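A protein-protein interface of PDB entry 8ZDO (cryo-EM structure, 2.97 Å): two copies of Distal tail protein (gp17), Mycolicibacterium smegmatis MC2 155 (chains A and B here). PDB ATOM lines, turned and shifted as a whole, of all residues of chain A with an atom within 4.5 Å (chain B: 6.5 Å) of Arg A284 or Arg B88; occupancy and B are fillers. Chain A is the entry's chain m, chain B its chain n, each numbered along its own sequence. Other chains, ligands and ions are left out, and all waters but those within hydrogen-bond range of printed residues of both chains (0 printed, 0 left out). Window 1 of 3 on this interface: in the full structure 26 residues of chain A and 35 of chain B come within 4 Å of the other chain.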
ATOM      1  N   TYR A  39       0.830  20.014 -24.403  1.00  0.00           N
ATOM      2  CA  TYR A  39       0.233  20.591 -23.205  1.00  0.00           C
ATOM      3  C   TYR A  39      -1.170  21.140 -23.446  1.00  0.00           C
ATOM      4  O   TYR A  39      -2.141  20.637 -22.876  1.00  0.00           O
ATOM      5  CB  TYR A  39       1.160  21.680 -22.658  1.00  0.00           C
ATOM      6  CG  TYR A  39       2.574  21.197 -22.447  1.00  0.00           C
ATOM      7  CD1 TYR A  39       2.897  20.383 -21.372  1.00  0.00           C
ATOM      8  CD2 TYR A  39       3.585  21.541 -23.330  1.00  0.00           C
ATOM      9  CE1 TYR A  39       4.185  19.936 -21.178  1.00  0.00           C
ATOM     10  CE2 TYR A  39       4.875  21.098 -23.143  1.00  0.00           C
ATOM     11  CZ  TYR A  39       5.169  20.296 -22.066  1.00  0.00           C
ATOM     12  OH  TYR A  39       6.456  19.853 -21.876  1.00  0.00           O
ATOM     13  N   ASP A  40      -1.304  22.147 -24.298  1.00  0.00           N
ATOM     14  CA  ASP A  40      -2.586  22.793 -24.532  1.00  0.00           C
ATOM     15  C   ASP A  40      -3.264  22.195 -25.754  1.00  0.00           C
ATOM     16  O   ASP A  40      -2.607  21.877 -26.750  1.00  0.00           O
ATOM     17  CB  ASP A  40      -2.417  24.302 -24.720  1.00  0.00           C
ATOM     18  CG  ASP A  40      -2.224  25.035 -23.410  1.00  0.00           C
ATOM     19  OD1 ASP A  40      -2.785  24.587 -22.390  1.00  0.00           O
ATOM     20  OD2 ASP A  40      -1.514  26.061 -23.398  1.00  0.00           O
ATOM     21  N   ARG A 108      -3.763  11.845 -15.966  1.00  0.00           N
ATOM     22  CA  ARG A 108      -4.593  12.096 -17.134  1.00  0.00           C
ATOM     23  C   ARG A 108      -3.965  11.426 -18.344  1.00  0.00           C
ATOM     24  O   ARG A 108      -2.751  11.495 -18.539  1.00  0.00           O
ATOM     25  CB  ARG A 108      -4.753  13.596 -17.382  1.00  0.00           C
ATOM     26  CG  ARG A 108      -5.465  14.311 -16.259  1.00  0.00           C
ATOM     27  CD  ARG A 108      -5.439  15.809 -16.444  1.00  0.00           C
ATOM     28  NE  ARG A 108      -5.586  16.497 -15.169  1.00  0.00           N
ATOM     29  CZ  ARG A 108      -5.749  17.805 -15.038  1.00  0.00           C
ATOM     30  NH1 ARG A 108      -5.782  18.604 -16.089  1.00  0.00           N
ATOM     31  NH2 ARG A 108      -5.891  18.321 -13.822  1.00  0.00           N
ATOM     32  N   TRP A 145      -7.065  15.853 -22.762  1.00  0.00           N
ATOM     33  CA  TRP A 145      -6.620  14.939 -21.722  1.00  0.00           C
ATOM     34  C   TRP A 145      -7.791  14.597 -20.817  1.00  0.00           C
ATOM     35  O   TRP A 145      -8.605  15.459 -20.479  1.00  0.00           O
ATOM     36  CB  TRP A 145      -5.492  15.561 -20.905  1.00  0.00           C
ATOM     37  CG  TRP A 145      -4.243  15.783 -21.677  1.00  0.00           C
ATOM     38  CD1 TRP A 145      -3.983  16.808 -22.531  1.00  0.00           C
ATOM     39  CD2 TRP A 145      -3.070  14.965 -21.661  1.00  0.00           C
ATOM     40  NE1 TRP A 145      -2.723  16.680 -23.054  1.00  0.00           N
ATOM     41  CE2 TRP A 145      -2.140  15.556 -22.534  1.00  0.00           C
ATOM     42  CE3 TRP A 145      -2.717  13.790 -20.993  1.00  0.00           C
ATOM     43  CZ2 TRP A 145      -0.883  15.012 -22.759  1.00  0.00           C
ATOM     44  CZ3 TRP A 145      -1.469  13.254 -21.219  1.00  0.00           C
ATOM     45  CH2 TRP A 145      -0.566  13.863 -22.093  1.00  0.00           C
ATOM     46  N   ASP A 172     -11.721  21.988 -17.643  1.00  0.00           N
ATOM     47  CA  ASP A 172     -11.597  23.184 -18.465  1.00  0.00           C
ATOM     48  C   ASP A 172     -12.638  23.255 -19.568  1.00  0.00           C
ATOM     49  O   ASP A 172     -12.964  24.353 -20.033  1.00  0.00           O
ATOM     50  CB  ASP A 172     -10.208  23.244 -19.107  1.00  0.00           C
ATOM     51  CG  ASP A 172      -9.088  23.159 -18.092  1.00  0.00           C
ATOM     52  OD1 ASP A 172      -9.288  23.601 -16.945  1.00  0.00           O
ATOM     53  OD2 ASP A 172      -8.005  22.649 -18.444  1.00  0.00           O
ATOM     54  N   TYR A 282      -9.977  17.384 -19.838  1.00  0.00           N
ATOM     55  CA  TYR A 282      -9.150  18.544 -19.565  1.00  0.00           C
ATOM     56  C   TYR A 282      -8.363  18.894 -20.816  1.00  0.00           C
ATOM     57  O   TYR A 282      -8.072  18.030 -21.646  1.00  0.00           O
ATOM     58  CB  TYR A 282      -8.191  18.291 -18.399  1.00  0.00           C
ATOM     59  CG  TYR A 282      -8.865  17.735 -17.172  1.00  0.00           C
ATOM     60  CD1 TYR A 282      -9.389  18.578 -16.206  1.00  0.00           C
ATOM     61  CD2 TYR A 282      -8.980  16.368 -16.978  1.00  0.00           C
ATOM     62  CE1 TYR A 282     -10.004  18.076 -15.085  1.00  0.00           C
ATOM     63  CE2 TYR A 282      -9.594  15.858 -15.858  1.00  0.00           C
ATOM     64  CZ  TYR A 282     -10.104  16.717 -14.915  1.00  0.00           C
ATOM     65  OH  TYR A 282     -10.719  16.217 -13.794  1.00  0.00           O
ATOM     66  N   SER A 283      -8.021  20.171 -20.947  1.00  0.00           N
ATOM     67  CA  SER A 283      -7.241  20.649 -22.077  1.00  0.00           C
ATOM     68  C   SER A 283      -5.749  20.676 -21.789  1.00  0.00           C
ATOM     69  O   SER A 283      -4.983  21.189 -22.609  1.00  0.00           O
ATOM     70  CB  SER A 283      -7.713  22.044 -22.488  1.00  0.00           C
ATOM     71  OG  SER A 283      -7.270  23.022 -21.567  1.00  0.00           O
ATOM     72  N   ARG A 284      -5.319  20.141 -20.647  1.00  0.00           N
ATOM     73  CA  ARG A 284      -3.942  20.253 -20.223  1.00  0.00           C
ATOM     74  C   ARG A 284      -3.578  19.016 -19.415  1.00  0.00           C
ATOM     75  O   ARG A 284      -4.442  18.479 -18.710  1.00  0.00           O
ATOM     76  CB  ARG A 284      -3.743  21.522 -19.390  1.00  0.00           C
ATOM     77  CG  ARG A 284      -2.315  21.987 -19.258  1.00  0.00           C
ATOM     78  CD  ARG A 284      -2.241  23.369 -18.645  1.00  0.00           C
ATOM     79  NE  ARG A 284      -2.036  24.400 -19.654  1.00  0.00           N
ATOM     80  CZ  ARG A 284      -1.460  25.570 -19.417  1.00  0.00           C
ATOM     81  NH1 ARG A 284      -1.021  25.889 -18.211  1.00  0.00           N
ATOM     82  NH2 ARG A 284      -1.316  26.437 -20.414  1.00  0.00           N
ATOM     83  N   PRO A 285      -2.336  18.529 -19.508  1.00  0.00           N
ATOM     84  CA  PRO A 285      -1.956  17.349 -18.715  1.00  0.00           C
ATOM     85  C   PRO A 285      -2.077  17.558 -17.219  1.00  0.00           C
ATOM     86  O   PRO A 285      -2.341  16.595 -16.491  1.00  0.00           O
ATOM     87  CB  PRO A 285      -0.501  17.100 -19.132  1.00  0.00           C
ATOM     88  CG  PRO A 285      -0.363  17.754 -20.441  1.00  0.00           C
ATOM     89  CD  PRO A 285      -1.251  18.947 -20.407  1.00  0.00           C
ATOM     90  N   TRP A 286      -1.872  18.778 -16.735  1.00  0.00           N
ATOM     91  CA  TRP A 286      -2.038  19.085 -15.323  1.00  0.00           C
ATOM     92  C   TRP A 286      -2.628  20.477 -15.184  1.00  0.00           C
ATOM     93  O   TRP A 286      -2.280  21.384 -15.943  1.00  0.00           O
ATOM     94  CB  TRP A 286      -0.711  18.996 -14.561  1.00  0.00           C
ATOM     95  CG  TRP A 286       0.361  19.897 -15.082  1.00  0.00           C
ATOM     96  CD1 TRP A 286       0.563  21.202 -14.756  1.00  0.00           C
ATOM     97  CD2 TRP A 286       1.390  19.554 -16.015  1.00  0.00           C
ATOM     98  NE1 TRP A 286       1.650  21.697 -15.430  1.00  0.00           N
ATOM     99  CE2 TRP A 286       2.177  20.703 -16.210  1.00  0.00           C
ATOM    100  CE3 TRP A 286       1.725  18.387 -16.704  1.00  0.00           C
ATOM    101  CZ2 TRP A 286       3.271  20.719 -17.066  1.00  0.00           C
ATOM    102  CZ3 TRP A 286       2.811  18.405 -17.552  1.00  0.00           C
ATOM    103  CH2 TRP A 286       3.572  19.563 -17.726  1.00  0.00           C
ATOM    104  N   ARG B  12     -10.842  36.602 -17.084  1.00  0.00           N
ATOM    105  CA  ARG B  12     -12.270  36.346 -17.190  1.00  0.00           C
ATOM    106  C   ARG B  12     -12.882  35.921 -15.862  1.00  0.00           C
ATOM    107  O   ARG B  12     -14.098  36.042 -15.684  1.00  0.00           O
ATOM    108  CB  ARG B  12     -12.515  35.272 -18.241  1.00  0.00           C
ATOM    109  CG  ARG B  12     -11.942  33.932 -17.845  1.00  0.00           C
ATOM    110  CD  ARG B  12     -12.310  32.890 -18.849  1.00  0.00           C
ATOM    111  NE  ARG B  12     -11.730  31.587 -18.557  1.00  0.00           N
ATOM    112  CZ  ARG B  12     -12.347  30.627 -17.886  1.00  0.00           C
ATOM    113  NH1 ARG B  12     -13.564  30.800 -17.396  1.00  0.00           N
ATOM    114  NH2 ARG B  12     -11.732  29.463 -17.709  1.00  0.00           N
ATOM    115  N   TRP B  17      -3.669  40.639 -12.269  1.00  0.00           N
ATOM    116  CA  TRP B  17      -2.243  40.430 -12.458  1.00  0.00           C
ATOM    117  C   TRP B  17      -1.602  41.749 -12.846  1.00  0.00           C
ATOM    118  O   TRP B  17      -2.150  42.491 -13.660  1.00  0.00           O
ATOM    119  CB  TRP B  17      -1.962  39.390 -13.548  1.00  0.00           C
ATOM    120  CG  TRP B  17      -2.764  38.138 -13.430  1.00  0.00           C
ATOM    121  CD1 TRP B  17      -4.064  37.964 -13.794  1.00  0.00           C
ATOM    122  CD2 TRP B  17      -2.316  36.876 -12.931  1.00  0.00           C
ATOM    123  NE1 TRP B  17      -4.457  36.677 -13.543  1.00  0.00           N
ATOM    124  CE2 TRP B  17      -3.400  35.987 -13.013  1.00  0.00           C
ATOM    125  CE3 TRP B  17      -1.101  36.412 -12.419  1.00  0.00           C
ATOM    126  CZ2 TRP B  17      -3.308  34.663 -12.602  1.00  0.00           C
ATOM    127  CZ3 TRP B  17      -1.013  35.099 -12.012  1.00  0.00           C
ATOM    128  CH2 TRP B  17      -2.107  34.239 -12.105  1.00  0.00           C
ATOM    129  N   VAL B  83       0.653  28.773  -9.940  1.00  0.00           N
ATOM    130  CA  VAL B  83       0.634  30.061 -10.632  1.00  0.00           C
ATOM    131  C   VAL B  83       0.366  29.869 -12.119  1.00  0.00           C
ATOM    132  O   VAL B  83      -0.389  30.632 -12.733  1.00  0.00           O
ATOM    133  CB  VAL B  83       1.954  30.814 -10.386  1.00  0.00           C
ATOM    134  CG1 VAL B  83       2.045  32.037 -11.272  1.00  0.00           C
ATOM    135  CG2 VAL B  83       2.070  31.210  -8.929  1.00  0.00           C
ATOM    136  N   ASP B  84       0.996  28.863 -12.725  1.00  0.00           N
ATOM    137  CA  ASP B  84       0.788  28.579 -14.142  1.00  0.00           C
ATOM    138  C   ASP B  84      -0.659  28.197 -14.421  1.00  0.00           C
ATOM    139  O   ASP B  84      -1.255  28.652 -15.408  1.00  0.00           O
ATOM    140  CB  ASP B  84       1.739  27.467 -14.579  1.00  0.00           C
ATOM    141  CG  ASP B  84       1.625  27.142 -16.052  1.00  0.00           C
ATOM    142  OD1 ASP B  84       2.081  27.953 -16.879  1.00  0.00           O
ATOM    143  OD2 ASP B  84       1.086  26.065 -16.382  1.00  0.00           O
ATOM    144  N   SER B  85      -1.247  27.371 -13.554  1.00  0.00           N
ATOM    145  CA  SER B  85      -2.651  27.013 -13.715  1.00  0.00           C
ATOM    146  C   SER B  85      -3.549  28.235 -13.583  1.00  0.00           C
ATOM    147  O   SER B  85      -4.517  28.381 -14.335  1.00  0.00           O
ATOM    148  CB  SER B  85      -3.040  25.951 -12.692  1.00  0.00           C
ATOM    149  OG  SER B  85      -4.370  25.513 -12.902  1.00  0.00           O
ATOM    150  N   LEU B  86      -3.251  29.120 -12.630  1.00  0.00           N
ATOM    151  CA  LEU B  86      -4.061  30.324 -12.468  1.00  0.00           C
ATOM    152  C   LEU B  86      -3.960  31.228 -13.690  1.00  0.00           C
ATOM    153  O   LEU B  86      -4.963  31.798 -14.140  1.00  0.00           O
ATOM    154  CB  LEU B  86      -3.636  31.076 -11.210  1.00  0.00           C
ATOM    155  CG  LEU B  86      -3.936  30.387  -9.880  1.00  0.00           C
ATOM    156  CD1 LEU B  86      -3.645  31.318  -8.721  1.00  0.00           C
ATOM    157  CD2 LEU B  86      -5.373  29.902  -9.844  1.00  0.00           C
ATOM    158  N   TRP B  87      -2.753  31.375 -14.238  1.00  0.00           N
ATOM    159  CA  TRP B  87      -2.589  32.179 -15.442  1.00  0.00           C
ATOM    160  C   TRP B  87      -3.388  31.597 -16.596  1.00  0.00           C
ATOM    161  O   TRP B  87      -4.036  32.336 -17.345  1.00  0.00           O
ATOM    162  CB  TRP B  87      -1.113  32.284 -15.818  1.00  0.00           C
ATOM    163  CG  TRP B  87      -0.896  33.072 -17.068  1.00  0.00           C
ATOM    164  CD1 TRP B  87      -0.569  32.584 -18.295  1.00  0.00           C
ATOM    165  CD2 TRP B  87      -1.009  34.490 -17.217  1.00  0.00           C
ATOM    166  NE1 TRP B  87      -0.463  33.609 -19.199  1.00  0.00           N
ATOM    167  CE2 TRP B  87      -0.729  34.790 -18.561  1.00  0.00           C
ATOM    168  CE3 TRP B  87      -1.315  35.534 -16.343  1.00  0.00           C
ATOM    169  CZ2 TRP B  87      -0.745  36.090 -19.051  1.00  0.00           C
ATOM    170  CZ3 TRP B  87      -1.330  36.817 -16.830  1.00  0.00           C
ATOM    171  CH2 TRP B  87      -1.047  37.087 -18.170  1.00  0.00           C
ATOM    172  N   ARG B  88      -3.359  30.273 -16.758  1.00  0.00           N
ATOM    173  CA  ARG B  88      -4.157  29.659 -17.815  1.00  0.00           C
ATOM    174  C   ARG B  88      -5.647  29.858 -17.563  1.00  0.00           C
ATOM    175  O   ARG B  88      -6.423  30.047 -18.506  1.00  0.00           O
ATOM    176  CB  ARG B  88      -3.821  28.174 -17.937  1.00  0.00           C
ATOM    177  CG  ARG B  88      -4.558  27.463 -19.060  1.00  0.00           C
ATOM    178  CD  ARG B  88      -4.391  28.182 -20.385  1.00  0.00           C
ATOM    179  NE  ARG B  88      -5.380  27.753 -21.368  1.00  0.00           N
ATOM    180  CZ  ARG B  88      -6.623  28.208 -21.429  1.00  0.00           C
ATOM    181  NH1 ARG B  88      -7.069  29.115 -20.577  1.00  0.00           N
ATOM    182  NH2 ARG B  88      -7.440  27.739 -22.366  1.00  0.00           N
ATOM    183  N   TRP B  89      -6.066  29.811 -16.298  1.00  0.00           N
ATOM    184  CA  TRP B  89      -7.473  30.011 -15.971  1.00  0.00           C
ATOM    185  C   TRP B  89      -7.921  31.437 -16.253  1.00  0.00           C
ATOM    186  O   TRP B  89      -9.106  31.676 -16.502  1.00  0.00           O
ATOM    187  CB  TRP B  89      -7.724  29.667 -14.504  1.00  0.00           C
ATOM    188  CG  TRP B  89      -8.023  28.225 -14.270  1.00  0.00           C
ATOM    189  CD1 TRP B  89      -7.251  27.327 -13.597  1.00  0.00           C
ATOM    190  CD2 TRP B  89      -9.180  27.509 -14.708  1.00  0.00           C
ATOM    191  NE1 TRP B  89      -7.855  26.097 -13.589  1.00  0.00           N
ATOM    192  CE2 TRP B  89      -9.042  26.182 -14.265  1.00  0.00           C
ATOM    193  CE3 TRP B  89     -10.322  27.864 -15.430  1.00  0.00           C
ATOM    194  CZ2 TRP B  89     -10.002  25.209 -14.519  1.00  0.00           C
ATOM    195  CZ3 TRP B  89     -11.270  26.897 -15.685  1.00  0.00           C
ATOM    196  CH2 TRP B  89     -11.106  25.585 -15.231  1.00  0.00           C
ATOM    197  N   ALA B  90      -6.997  32.393 -16.206  1.00  0.00           N
ATOM    198  CA  ALA B  90      -7.353  33.788 -16.447  1.00  0.00           C
ATOM    199  C   ALA B  90      -7.699  34.092 -17.902  1.00  0.00           C
ATOM    200  O   ALA B  90      -7.957  35.259 -18.212  1.00  0.00           O
ATOM    201  CB  ALA B  90      -6.211  34.700 -16.000  1.00  0.00           C
ATOM    202  N   TRP B  91      -7.723  33.105 -18.794  1.00  0.00           N
ATOM    203  CA  TRP B  91      -7.913  33.345 -20.217  1.00  0.00           C
ATOM    204  C   TRP B  91      -8.981  32.417 -20.779  1.00  0.00           C
ATOM    205  O   TRP B  91      -9.311  31.386 -20.189  1.00  0.00           O
ATOM    206  CB  TRP B  91      -6.610  33.144 -20.993  1.00  0.00           C
ATOM    207  CG  TRP B  91      -5.575  34.177 -20.724  1.00  0.00           C
ATOM    208  CD1 TRP B  91      -4.529  34.080 -19.859  1.00  0.00           C
ATOM    209  CD2 TRP B  91      -5.478  35.468 -21.330  1.00  0.00           C
ATOM    210  NE1 TRP B  91      -3.787  35.234 -19.884  1.00  0.00           N
ATOM    211  CE2 TRP B  91      -4.349  36.102 -20.782  1.00  0.00           C
ATOM    212  CE3 TRP B  91      -6.235  36.150 -22.284  1.00  0.00           C
ATOM    213  CZ2 TRP B  91      -3.961  37.383 -21.156  1.00  0.00           C
ATOM    214  CZ3 TRP B  91      -5.851  37.417 -22.649  1.00  0.00           C
ATOM    215  CH2 TRP B  91      -4.723  38.021 -22.091  1.00  0.00           C
ATOM    216  N   ASP B  92      -9.513  32.794 -21.941  1.00  0.00           N
ATOM    217  CA  ASP B  92     -10.474  31.967 -22.660  1.00  0.00           C
ATOM    218  C   ASP B  92     -10.529  32.411 -24.113  1.00  0.00           C
ATOM    219  O   ASP B  92      -9.922  33.409 -24.505  1.00  0.00           O
ATOM    220  CB  ASP B  92     -11.869  32.046 -22.041  1.00  0.00           C
ATOM    221  CG  ASP B  92     -12.683  30.791 -22.273  1.00  0.00           C
ATOM    222  OD1 ASP B  92     -12.084  29.704 -22.404  1.00  0.00           O
ATOM    223  OD2 ASP B  92     -13.926  30.891 -22.324  1.00  0.00           O
ATOM    224  N   TYR B  93     -11.276  31.649 -24.907  1.00  0.00           N
ATOM    225  CA  TYR B  93     -11.595  32.002 -26.283  1.00  0.00           C
ATOM    226  C   TYR B  93     -12.979  32.618 -26.421  1.00  0.00           C
ATOM    227  O   TYR B  93     -13.145  33.596 -27.154  1.00  0.00           O
ATOM    228  CB  TYR B  93     -11.505  30.770 -27.187  1.00  0.00           C
ATOM    229  CG  TYR B  93     -10.327  29.867 -26.906  1.00  0.00           C
ATOM    230  CD1 TYR B  93      -9.118  30.050 -27.558  1.00  0.00           C
ATOM    231  CD2 TYR B  93     -10.428  28.823 -26.000  1.00  0.00           C
ATOM    232  CE1 TYR B  93      -8.042  29.229 -27.307  1.00  0.00           C
ATOM    233  CE2 TYR B  93      -9.358  27.998 -25.742  1.00  0.00           C
ATOM    234  CZ  TYR B  93      -8.167  28.205 -26.399  1.00  0.00           C
ATOM    235  OH  TYR B  93      -7.096  27.382 -26.146  1.00  0.00           O
ATOM    236  N   LEU B 114      -8.150  34.760 -26.229  1.00  0.00           N
ATOM    237  CA  LEU B 114      -7.162  33.847 -26.786  1.00  0.00           C
ATOM    238  C   LEU B 114      -7.458  33.569 -28.252  1.00  0.00           C
ATOM    239  O   LEU B 114      -8.492  32.984 -28.585  1.00  0.00           O
ATOM    240  CB  LEU B 114      -7.153  32.544 -25.992  1.00  0.00           C
ATOM    241  CG  LEU B 114      -6.282  32.511 -24.743  1.00  0.00           C
ATOM    242  CD1 LEU B 114      -6.446  31.185 -24.041  1.00  0.00           C
ATOM    243  CD2 LEU B 114      -4.839  32.740 -25.120  1.00  0.00           C
ATOM    244  N   GLU B 117      -4.312  28.464 -28.889  1.00  0.00           N
ATOM    245  CA  GLU B 117      -3.828  27.900 -27.641  1.00  0.00           C
ATOM    246  C   GLU B 117      -2.471  28.502 -27.280  1.00  0.00           C
ATOM    247  O   GLU B 117      -1.663  28.795 -28.165  1.00  0.00           O
ATOM    248  CB  GLU B 117      -3.730  26.376 -27.742  1.00  0.00           C
ATOM    249  CG  GLU B 117      -2.512  25.852 -28.479  1.00  0.00           C
ATOM    250  CD  GLU B 117      -2.610  26.041 -29.979  1.00  0.00           C
ATOM    251  OE1 GLU B 117      -3.735  26.226 -30.485  1.00  0.00           O
ATOM    252  OE2 GLU B 117      -1.559  26.003 -30.655  1.00  0.00           O
ATOM    253  N   PRO B 118      -2.207  28.728 -25.997  1.00  0.00           N
ATOM    254  CA  PRO B 118      -0.911  29.281 -25.596  1.00  0.00           C
ATOM    255  C   PRO B 118       0.211  28.284 -25.826  1.00  0.00           C
ATOM    256  O   PRO B 118       0.002  27.072 -25.896  1.00  0.00           O
ATOM    257  CB  PRO B 118      -1.092  29.572 -24.102  1.00  0.00           C
ATOM    258  CG  PRO B 118      -2.570  29.566 -23.876  1.00  0.00           C
ATOM    259  CD  PRO B 118      -3.130  28.598 -24.860  1.00  0.00           C
ATOM    260  N   PRO B 120       3.330  27.131 -23.923  1.00  0.00           N
ATOM    261  CA  PRO B 120       4.052  27.266 -22.654  1.00  0.00           C
ATOM    262  C   PRO B 120       5.376  26.519 -22.602  1.00  0.00           C
ATOM    263  O   PRO B 120       5.667  25.670 -23.451  1.00  0.00           O
ATOM    264  CB  PRO B 120       3.054  26.699 -21.643  1.00  0.00           C
ATOM    265  CG  PRO B 120       2.296  25.664 -22.417  1.00  0.00           C
ATOM    266  CD  PRO B 120       2.363  26.023 -23.884  1.00  0.00           C
ATOM    267  N   TYR B 121       6.188  26.870 -21.605  1.00  0.00           N
ATOM    268  CA  TYR B 121       7.323  26.082 -21.134  1.00  0.00           C
ATOM    269  C   TYR B 121       8.484  26.053 -22.119  1.00  0.00           C
ATOM    270  O   TYR B 121       8.357  26.490 -23.266  1.00  0.00           O
ATOM    271  CB  TYR B 121       6.875  24.655 -20.803  1.00  0.00           C
ATOM    272  CG  TYR B 121       5.582  24.590 -20.022  1.00  0.00           C
ATOM    273  CD1 TYR B 121       5.290  25.529 -19.043  1.00  0.00           C
ATOM    274  CD2 TYR B 121       4.651  23.594 -20.269  1.00  0.00           C
ATOM    275  CE1 TYR B 121       4.114  25.476 -18.339  1.00  0.00           C
ATOM    276  CE2 TYR B 121       3.471  23.534 -19.564  1.00  0.00           C
ATOM    277  CZ  TYR B 121       3.208  24.477 -18.600  1.00  0.00           C
ATOM    278  OH  TYR B 121       2.030  24.419 -17.896  1.00  0.00           O
ATOM    279  N   ILE B 134       5.390  31.680 -21.204  1.00  0.00           N
ATOM    280  CA  ILE B 134       4.152  31.346 -21.883  1.00  0.00           C
ATOM    281  C   ILE B 134       3.982  32.343 -23.018  1.00  0.00           C
ATOM    282  O   ILE B 134       3.999  33.558 -22.785  1.00  0.00           O
ATOM    283  CB  ILE B 134       2.955  31.388 -20.927  1.00  0.00           C
ATOM    284  CG1 ILE B 134       3.127  30.342 -19.830  1.00  0.00           C
ATOM    285  CG2 ILE B 134       1.680  31.126 -21.683  1.00  0.00           C
ATOM    286  CD1 ILE B 134       2.142  30.485 -18.713  1.00  0.00           C
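The guanidinium group of Arg A284 is in hydrogen-bond range of the side-chain hydroxyl of Tyr B121. OD2 of Asp A40 sits close to O of Pro B118. NH1 of Arg A284 is in salt-bridge range of OD2 of Asp B84 (2.8 Å).
No position is printed for both chains.
Tyr B121 touches Tyr A39. Asp A40 touches Glu B117. Asp A40 touches Pro B120. Trp B89 touches Asp A172. CD of Arg B88 touches NH2 of Arg A284, at 3.5 Å. OH of Tyr B121 touches NE1 of Trp A286 (3.7 Å).
NH1 of Arg B88 is in hydrogen-bond range of O of Trp B91, at 3.2 Å. The guanidinium group (NE) of Arg B12 is in hydrogen-bond range of the backbone carbonyl oxygen (O) of Trp B89, 3.3 Å away. The side-chain carboxylate of Asp A172 sits at hydrogen-bond distance from the side-chain hydroxyl of Ser A283, 3.2 Å away. The side-chain carboxylate (OD2) of Asp B84 is in hydrogen-bond range of the side-chain hydroxyl (OH) of Tyr B121, at 2.4 Å. OD1 of Asp A40 is in salt-bridge range of NE of Arg A284 (2.8 Å). O of Arg A284 sits at hydrogen-bond distance from NH1 of Arg A108 (2.9 Å).
Hydrophobic or aromatic side chains of chain B within 4 Å of the printed part of chain A: Trp B89, Pro B118, Pro B120 and Tyr B121. Of the 10 printed residues of chain A, 5 touch a printed residue of chain B. Printed residues of chain A that touch a printed residue of chain B: Tyr A39, Asp A40, Asp A172, Arg A284 and Trp A286. Hydrophobic or aromatic side chains of chain A within 4 Å of the printed part of chain B: Tyr A39 and Trp A286.
Of the printed residues of chain B, Arg A284 touches Asp B84 (2.8 Å), Arg B88 (3.5 Å) and Tyr B121 (3.4 Å). Arg B88 touches just one residue of chain A: Arg A284 (3.5 Å). Printed residues of chain A within 4 Å of Pro B120: Asp A40 (3.9 Å). Printed residues of chain B within 4 Å of Tyr A39: Tyr B121. Arg B12 touches none of the printed residues of chain A. Tyr B93 touches none of the printed residues of chain A. The nearest residue of chain B that does not touch Arg A284 is Pro B120 (4.2 Å). The nearest printed residue of chain B that does not touch Asp A172 is Arg B12 (5.7 Å).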
